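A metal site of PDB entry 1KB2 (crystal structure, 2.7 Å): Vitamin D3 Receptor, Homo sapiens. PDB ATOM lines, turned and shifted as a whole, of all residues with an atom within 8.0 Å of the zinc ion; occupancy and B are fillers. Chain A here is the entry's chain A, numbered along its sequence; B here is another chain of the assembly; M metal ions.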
ATOM      1  N   ILE A   8     -29.596   1.748  10.827  1.00  0.00           N
ATOM      2  CA  ILE A   8     -28.390   1.100  11.324  1.00  0.00           C
ATOM      3  C   ILE A   8     -27.184   1.258  10.405  1.00  0.00           C
ATOM      4  O   ILE A   8     -27.320   1.310   9.206  1.00  0.00           O
ATOM      5  CB  ILE A   8     -28.632  -0.419  11.652  1.00  0.00           C
ATOM      6  CG1 ILE A   8     -29.336  -1.115  10.466  1.00  0.00           C
ATOM      7  CG2 ILE A   8     -29.504  -0.537  12.894  1.00  0.00           C
ATOM      8  CD1 ILE A   8     -29.690  -2.612  10.655  1.00  0.00           C
ATOM      9  N   CYS A   9     -26.019   1.356  11.007  1.00  0.00           N
ATOM     10  CA  CYS A   9     -24.771   1.491  10.261  1.00  0.00           C
ATOM     11  C   CYS A   9     -24.488   0.172   9.546  1.00  0.00           C
ATOM     12  O   CYS A   9     -24.486  -0.903  10.152  1.00  0.00           O
ATOM     13  CB  CYS A   9     -23.610   1.818  11.210  1.00  0.00           C
ATOM     14  SG  CYS A   9     -22.046   2.078  10.388  1.00  0.00           S
ATOM     15  N   GLY A  10     -24.259   0.230   8.255  1.00  0.00           N
ATOM     16  CA  GLY A  10     -23.993  -0.977   7.517  1.00  0.00           C
ATOM     17  C   GLY A  10     -22.607  -1.521   7.731  1.00  0.00           C
ATOM     18  O   GLY A  10     -22.236  -2.530   7.153  1.00  0.00           O
ATOM     19  N   VAL A  11     -21.807  -0.875   8.564  1.00  0.00           N
ATOM     20  CA  VAL A  11     -20.475  -1.384   8.798  1.00  0.00           C
ATOM     21  C   VAL A  11     -20.416  -1.971  10.188  1.00  0.00           C
ATOM     22  O   VAL A  11     -20.050  -3.128  10.352  1.00  0.00           O
ATOM     23  CB  VAL A  11     -19.401  -0.248   8.590  1.00  0.00           C
ATOM     24  CG1 VAL A  11     -18.045  -0.646   9.092  1.00  0.00           C
ATOM     25  CG2 VAL A  11     -19.318   0.086   7.114  1.00  0.00           C
ATOM     26  N   CYS A  12     -20.852  -1.222  11.198  1.00  0.00           N
ATOM     27  CA  CYS A  12     -20.750  -1.726  12.542  1.00  0.00           C
ATOM     28  C   CYS A  12     -22.033  -2.056  13.286  1.00  0.00           C
ATOM     29  O   CYS A  12     -22.002  -2.578  14.414  1.00  0.00           O
ATOM     30  CB  CYS A  12     -19.941  -0.762  13.356  1.00  0.00           C
ATOM     31  SG  CYS A  12     -20.810   0.705  13.648  1.00  0.00           S
ATOM     32  N   GLY A  13     -23.158  -1.741  12.672  1.00  0.00           N
ATOM     33  CA  GLY A  13     -24.441  -2.036  13.287  1.00  0.00           C
ATOM     34  C   GLY A  13     -24.987  -0.903  14.124  1.00  0.00           C
ATOM     35  O   GLY A  13     -26.190  -0.788  14.355  1.00  0.00           O
ATOM     36  N   ASP A  14     -24.072  -0.051  14.547  1.00  0.00           N
ATOM     37  CA  ASP A  14     -24.436   1.089  15.342  1.00  0.00           C
ATOM     38  C   ASP A  14     -25.485   2.006  14.683  1.00  0.00           C
ATOM     39  O   ASP A  14     -25.793   1.909  13.506  1.00  0.00           O
ATOM     40  CB  ASP A  14     -23.190   1.863  15.654  1.00  0.00           C
ATOM     41  CG  ASP A  14     -23.396   2.807  16.773  1.00  0.00           C
ATOM     42  OD1 ASP A  14     -22.492   3.634  17.022  1.00  0.00           O
ATOM     43  OD2 ASP A  14     -24.468   2.691  17.408  1.00  0.00           O
ATOM     44  N   ARG A  15     -26.011   2.923  15.471  1.00  0.00           N
ATOM     45  CA  ARG A  15     -27.035   3.817  14.952  1.00  0.00           C
ATOM     46  C   ARG A  15     -26.495   4.716  13.868  1.00  0.00           C
ATOM     47  O   ARG A  15     -25.649   5.576  14.123  1.00  0.00           O
ATOM     48  CB  ARG A  15     -27.564   4.686  16.087  1.00  0.00           C
ATOM     49  CG  ARG A  15     -28.817   5.483  15.746  1.00  0.00           C
ATOM     50  CD  ARG A  15     -29.247   6.337  16.954  1.00  0.00           C
ATOM     51  NE  ARG A  15     -28.245   7.346  17.294  1.00  0.00           N
ATOM     52  CZ  ARG A  15     -27.998   8.425  16.546  1.00  0.00           C
ATOM     53  NH1 ARG A  15     -28.690   8.624  15.418  1.00  0.00           N
ATOM     54  NH2 ARG A  15     -27.071   9.296  16.915  1.00  0.00           N
ATOM     55  N   ALA A  16     -27.004   4.516  12.661  1.00  0.00           N
ATOM     56  CA  ALA A  16     -26.614   5.324  11.525  1.00  0.00           C
ATOM     57  C   ALA A  16     -27.143   6.743  11.751  1.00  0.00           C
ATOM     58  O   ALA A  16     -28.009   6.943  12.586  1.00  0.00           O
ATOM     59  CB  ALA A  16     -27.208   4.766  10.265  1.00  0.00           C
ATOM     60  N   MET A  24     -25.293   4.163   4.203  1.00  0.00           N
ATOM     61  CA  MET A  24     -25.887   4.453   5.504  1.00  0.00           C
ATOM     62  C   MET A  24     -24.862   4.068   6.549  1.00  0.00           C
ATOM     63  O   MET A  24     -24.521   2.919   6.627  1.00  0.00           O
ATOM     64  CB  MET A  24     -27.153   3.610   5.662  1.00  0.00           C
ATOM     65  CG  MET A  24     -27.905   3.865   6.941  1.00  0.00           C
ATOM     66  SD  MET A  24     -28.391   5.634   7.130  1.00  0.00           S
ATOM     67  CE  MET A  24     -29.374   5.790   5.558  1.00  0.00           C
ATOM     68  N   THR A  25     -24.370   5.004   7.366  1.00  0.00           N
ATOM     69  CA  THR A  25     -23.347   4.655   8.336  1.00  0.00           C
ATOM     70  C   THR A  25     -23.463   5.487   9.613  1.00  0.00           C
ATOM     71  O   THR A  25     -24.220   6.428   9.639  1.00  0.00           O
ATOM     72  CB  THR A  25     -21.911   4.895   7.739  1.00  0.00           C
ATOM     73  OG1 THR A  25     -21.667   6.296   7.669  1.00  0.00           O
ATOM     74  CG2 THR A  25     -21.791   4.352   6.328  1.00  0.00           C
ATOM     75  N   CYS A  26     -22.702   5.141  10.660  1.00  0.00           N
ATOM     76  CA  CYS A  26     -22.733   5.901  11.905  1.00  0.00           C
ATOM     77  C   CYS A  26     -21.692   6.999  11.763  1.00  0.00           C
ATOM     78  O   CYS A  26     -21.057   7.065  10.737  1.00  0.00           O
ATOM     79  CB  CYS A  26     -22.384   5.001  13.077  1.00  0.00           C
ATOM     80  SG  CYS A  26     -20.693   4.332  13.130  1.00  0.00           S
ATOM     81  N   GLU A  27     -21.477   7.850  12.772  1.00  0.00           N
ATOM     82  CA  GLU A  27     -20.471   8.911  12.665  1.00  0.00           C
ATOM     83  C   GLU A  27     -19.074   8.416  12.796  1.00  0.00           C
ATOM     84  O   GLU A  27     -18.169   9.072  12.300  1.00  0.00           O
ATOM     85  CB  GLU A  27     -20.621   9.962  13.720  1.00  0.00           C
ATOM     86  CG  GLU A  27     -21.251  11.220  13.227  1.00  0.00           C
ATOM     87  CD  GLU A  27     -20.285  12.117  12.479  1.00  0.00           C
ATOM     88  OE1 GLU A  27     -19.255  12.547  13.043  1.00  0.00           O
ATOM     89  OE2 GLU A  27     -20.587  12.416  11.307  1.00  0.00           O
ATOM     90  N   GLY A  28     -18.875   7.298  13.492  1.00  0.00           N
ATOM     91  CA  GLY A  28     -17.523   6.788  13.651  1.00  0.00           C
ATOM     92  C   GLY A  28     -16.992   6.282  12.315  1.00  0.00           C
ATOM     93  O   GLY A  28     -15.877   6.620  11.882  1.00  0.00           O
ATOM     94  N   CYS A  29     -17.821   5.478  11.669  1.00  0.00           N
ATOM     95  CA  CYS A  29     -17.428   4.906  10.403  1.00  0.00           C
ATOM     96  C   CYS A  29     -17.388   5.905   9.271  1.00  0.00           C
ATOM     97  O   CYS A  29     -16.719   5.691   8.272  1.00  0.00           O
ATOM     98  CB  CYS A  29     -18.351   3.746  10.073  1.00  0.00           C
ATOM     99  SG  CYS A  29     -18.140   2.380  11.202  1.00  0.00           S
ATOM    100  N   LYS A  30     -18.133   6.993   9.417  1.00  0.00           N
ATOM    101  CA  LYS A  30     -18.095   8.040   8.421  1.00  0.00           C
ATOM    102  C   LYS A  30     -16.648   8.512   8.477  1.00  0.00           C
ATOM    103  O   LYS A  30     -15.934   8.494   7.470  1.00  0.00           O
ATOM    104  CB  LYS A  30     -19.010   9.179   8.839  1.00  0.00           C
ATOM    105  CG  LYS A  30     -18.691  10.495   8.180  1.00  0.00           C
ATOM    106  CD  LYS A  30     -19.573  11.564   8.699  1.00  0.00           C
ATOM    107  CE  LYS A  30     -18.803  12.845   8.801  1.00  0.00           C
ATOM    108  NZ  LYS A  30     -19.625  13.871   9.490  1.00  0.00           N
ATOM    109  N   PHE A  32     -13.928   7.195  10.075  1.00  0.00           N
ATOM    110  CA  PHE A  32     -12.874   6.199   9.892  1.00  0.00           C
ATOM    111  C   PHE A  32     -12.605   6.034   8.385  1.00  0.00           C
ATOM    112  O   PHE A  32     -11.478   5.837   7.952  1.00  0.00           O
ATOM    113  CB  PHE A  32     -13.322   4.853  10.481  1.00  0.00           C
ATOM    114  CG  PHE A  32     -12.470   3.708  10.102  1.00  0.00           C
ATOM    115  CD1 PHE A  32     -11.184   3.590  10.620  1.00  0.00           C
ATOM    116  CD2 PHE A  32     -12.916   2.771   9.176  1.00  0.00           C
ATOM    117  CE1 PHE A  32     -10.352   2.575  10.215  1.00  0.00           C
ATOM    118  CE2 PHE A  32     -12.132   1.752   8.759  1.00  0.00           C
ATOM    119  CZ  PHE A  32     -10.830   1.641   9.262  1.00  0.00           C
ATOM    120  N   ILE A  53     -17.762  -7.242  12.365  1.00  0.00           N
ATOM    121  CA  ILE A  53     -17.741  -5.904  12.929  1.00  0.00           C
ATOM    122  C   ILE A  53     -18.961  -5.516  13.755  1.00  0.00           C
ATOM    123  O   ILE A  53     -20.106  -5.697  13.344  1.00  0.00           O
ATOM    124  CB  ILE A  53     -17.523  -4.851  11.807  1.00  0.00           C
ATOM    125  CG1 ILE A  53     -16.277  -5.176  10.975  1.00  0.00           C
ATOM    126  CG2 ILE A  53     -17.343  -3.484  12.439  1.00  0.00           C
ATOM    127  CD1 ILE A  53     -15.015  -5.224  11.824  1.00  0.00           C
ATOM    128  N   THR A  54     -18.723  -4.985  14.948  1.00  0.00           N
ATOM    129  CA  THR A  54     -19.838  -4.543  15.787  1.00  0.00           C
ATOM    130  C   THR A  54     -19.558  -3.165  16.373  1.00  0.00           C
ATOM    131  O   THR A  54     -18.401  -2.696  16.418  1.00  0.00           O
ATOM    132  CB  THR A  54     -20.155  -5.495  16.993  1.00  0.00           C
ATOM    133  OG1 THR A  54     -19.105  -5.428  17.987  1.00  0.00           O
ATOM    134  CG2 THR A  54     -20.355  -6.891  16.519  1.00  0.00           C
ATOM    135  N   LYS A  55     -20.632  -2.517  16.806  1.00  0.00           N
ATOM    136  CA  LYS A  55     -20.496  -1.228  17.438  1.00  0.00           C
ATOM    137  C   LYS A  55     -19.352  -1.199  18.482  1.00  0.00           C
ATOM    138  O   LYS A  55     -18.723  -0.172  18.669  1.00  0.00           O
ATOM    139  CB  LYS A  55     -21.829  -0.864  18.096  1.00  0.00           C
ATOM    140  CG  LYS A  55     -21.678  -0.079  19.392  1.00  0.00           C
ATOM    141  CD  LYS A  55     -22.177   1.353  19.285  1.00  0.00           C
ATOM    142  CE  LYS A  55     -21.833   2.066  20.557  1.00  0.00           C
ATOM    143  NZ  LYS A  55     -20.451   1.617  20.961  1.00  0.00           N
ATOM    144  N   ARG A  58     -15.303  -2.589  16.559  1.00  0.00           N
ATOM    145  CA  ARG A  58     -14.834  -1.964  15.323  1.00  0.00           C
ATOM    146  C   ARG A  58     -13.466  -1.310  15.341  1.00  0.00           C
ATOM    147  O   ARG A  58     -12.863  -1.137  14.306  1.00  0.00           O
ATOM    148  CB  ARG A  58     -15.857  -0.967  14.823  1.00  0.00           C
ATOM    149  CG  ARG A  58     -15.895   0.297  15.614  1.00  0.00           C
ATOM    150  CD  ARG A  58     -17.182   1.068  15.382  1.00  0.00           C
ATOM    151  NE  ARG A  58     -17.187   2.246  16.246  1.00  0.00           N
ATOM    152  CZ  ARG A  58     -18.254   2.952  16.573  1.00  0.00           C
ATOM    153  NH1 ARG A  58     -19.455   2.613  16.106  1.00  0.00           N
ATOM    154  NH2 ARG A  58     -18.115   3.979  17.400  1.00  0.00           N
ATOM    155  N   ARG A  65     -12.826  -3.490   9.041  1.00  0.00           N
ATOM    156  CA  ARG A  65     -13.762  -2.372   9.028  1.00  0.00           C
ATOM    157  C   ARG A  65     -13.724  -1.623   7.663  1.00  0.00           C
ATOM    158  O   ARG A  65     -14.787  -1.328   7.046  1.00  0.00           O
ATOM    159  CB  ARG A  65     -13.400  -1.398  10.114  1.00  0.00           C
ATOM    160  CG  ARG A  65     -14.455  -0.356  10.380  1.00  0.00           C
ATOM    161  CD  ARG A  65     -14.010   0.511  11.480  1.00  0.00           C
ATOM    162  NE  ARG A  65     -14.979   1.505  11.899  1.00  0.00           N
ATOM    163  CZ  ARG A  65     -14.719   2.382  12.873  1.00  0.00           C
ATOM    164  NH1 ARG A  65     -13.533   2.335  13.473  1.00  0.00           N
ATOM    165  NH2 ARG A  65     -15.589   3.280  13.245  1.00  0.00           N
ATOM    166  N   CYS A  69     -16.478  -1.086   4.664  1.00  0.00           N
ATOM    167  CA  CYS A  69     -16.955   0.215   4.169  1.00  0.00           C
ATOM    168  C   CYS A  69     -17.030   0.206   2.671  1.00  0.00           C
ATOM    169  O   CYS A  69     -18.034   0.638   2.076  1.00  0.00           O
ATOM    170  CB  CYS A  69     -16.009   1.342   4.536  1.00  0.00           C
ATOM    171  SG  CYS A  69     -15.928   1.814   6.270  1.00  0.00           S
ATOM    172  N   ILE A  72     -19.832  -2.170   1.455  1.00  0.00           N
ATOM    173  CA  ILE A  72     -21.234  -1.796   1.485  1.00  0.00           C
ATOM    174  C   ILE A  72     -21.491  -0.661   0.547  1.00  0.00           C
ATOM    175  O   ILE A  72     -22.601  -0.168   0.443  1.00  0.00           O
ATOM    176  CB  ILE A  72     -21.769  -1.415   2.862  1.00  0.00           C
ATOM    177  CG1 ILE A  72     -21.201  -0.112   3.375  1.00  0.00           C
ATOM    178  CG2 ILE A  72     -21.425  -2.471   3.799  1.00  0.00           C
ATOM    179  CD1 ILE A  72     -21.759   0.301   4.715  1.00  0.00           C
ATOM    180  N   MET A  74     -19.327   2.360   0.241  1.00  0.00           N
ATOM    181  CA  MET A  74     -18.799   3.706   0.508  1.00  0.00           C
ATOM    182  C   MET A  74     -17.789   4.111  -0.572  1.00  0.00           C
ATOM    183  O   MET A  74     -17.007   3.288  -1.027  1.00  0.00           O
ATOM    184  CB  MET A  74     -18.160   3.762   1.887  1.00  0.00           C
ATOM    185  CG  MET A  74     -19.184   3.857   3.013  1.00  0.00           C
ATOM    186  SD  MET A  74     -18.467   3.696   4.612  1.00  0.00           S
ATOM    187  CE  MET A  74     -18.556   5.383   5.187  1.00  0.00           C
ATOM    188  P    DG B  11     -14.547   4.941  16.390  1.00  0.00           P
ATOM    189  OP1  DG B  11     -15.218   3.827  17.098  1.00  0.00           O
ATOM    190  OP2  DG B  11     -14.451   4.893  14.915  1.00  0.00           O
ATOM    191  O5'  DG B  11     -15.379   6.182  16.896  1.00  0.00           O
ATOM    192  C5'  DG B  11     -15.579   6.375  18.304  1.00  0.00           C
ATOM    193  C4'  DG B  11     -16.213   7.720  18.589  1.00  0.00           C
ATOM    194  O4'  DG B  11     -15.279   8.785  18.385  1.00  0.00           O
ATOM    195  C3'  DG B  11     -17.429   8.085  17.762  1.00  0.00           C
ATOM    196  O3'  DG B  11     -18.163   8.965  18.570  1.00  0.00           O
ATOM    197  C2'  DG B  11     -16.815   8.937  16.674  1.00  0.00           C
ATOM    198  C1'  DG B  11     -15.863   9.730  17.524  1.00  0.00           C
ATOM    199  N9   DG B  11     -14.796  10.406  16.813  1.00  0.00           N
ATOM    200  C8   DG B  11     -14.308  10.078  15.581  1.00  0.00           C
ATOM    201  N7   DG B  11     -13.327  10.845  15.203  1.00  0.00           N
ATOM    202  C5   DG B  11     -13.164  11.751  16.244  1.00  0.00           C
ATOM    203  C6   DG B  11     -12.272  12.831  16.372  1.00  0.00           C
ATOM    204  O6   DG B  11     -11.429  13.243  15.548  1.00  0.00           O
ATOM    205  N1   DG B  11     -12.426  13.484  17.590  1.00  0.00           N
ATOM    206  C2   DG B  11     -13.345  13.141  18.534  1.00  0.00           C
ATOM    207  N2   DG B  11     -13.316  13.876  19.656  1.00  0.00           N
ATOM    208  N3   DG B  11     -14.225  12.147  18.416  1.00  0.00           N
ATOM    209  C4   DG B  11     -14.064  11.484  17.251  1.00  0.00           C
HETATM  210 ZN    ZN M   1     -20.425   2.252  11.958  1.00  0.00          ZN
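The side-chain sulfur (SG) of Cys 9 sits close to the backbone NH (N) of Val 11 of chain A (3.5 Å). N of Cys 9 is in hydrogen-bond range of O of Asp 14 (2.6 Å). The side-chain sulfur of Cys 12 lies close to the guanidinium group of Arg 58, at 3.4 Å. The backbone NH (N) of Asp 14 sits close to the side-chain sulfur (SG) of Cys 12. O of Cys 12 sits at hydrogen-bond distance from N of Lys 55 (2.8 Å). The guanidinium group (NH1) of Arg 58 lies close to the side-chain sulfur (SG) of Cys 26, 3.7 Å away. The side-chain sulfur (SG) of Cys 26 sits close to the backbone NH (N) of Gly 28, 3.5 Å away. SG of Cys 29 sits close to NE of Arg 65, 3.4 Å away.
Four residues have an atom within 4 Å of the zinc ion: Cys 9, Cys 12, Cys 26 and Cys 29. The nearest printed residue that does not touch the zinc ion is Arg 58 (4.3 Å).
The zinc ion is bound by SG of Cys 9 (2.3 Å), SG of Cys 12 (2.3 Å), SG of Cys 26 (2.4 Å) and SG of Cys 29 (2.4 Å).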
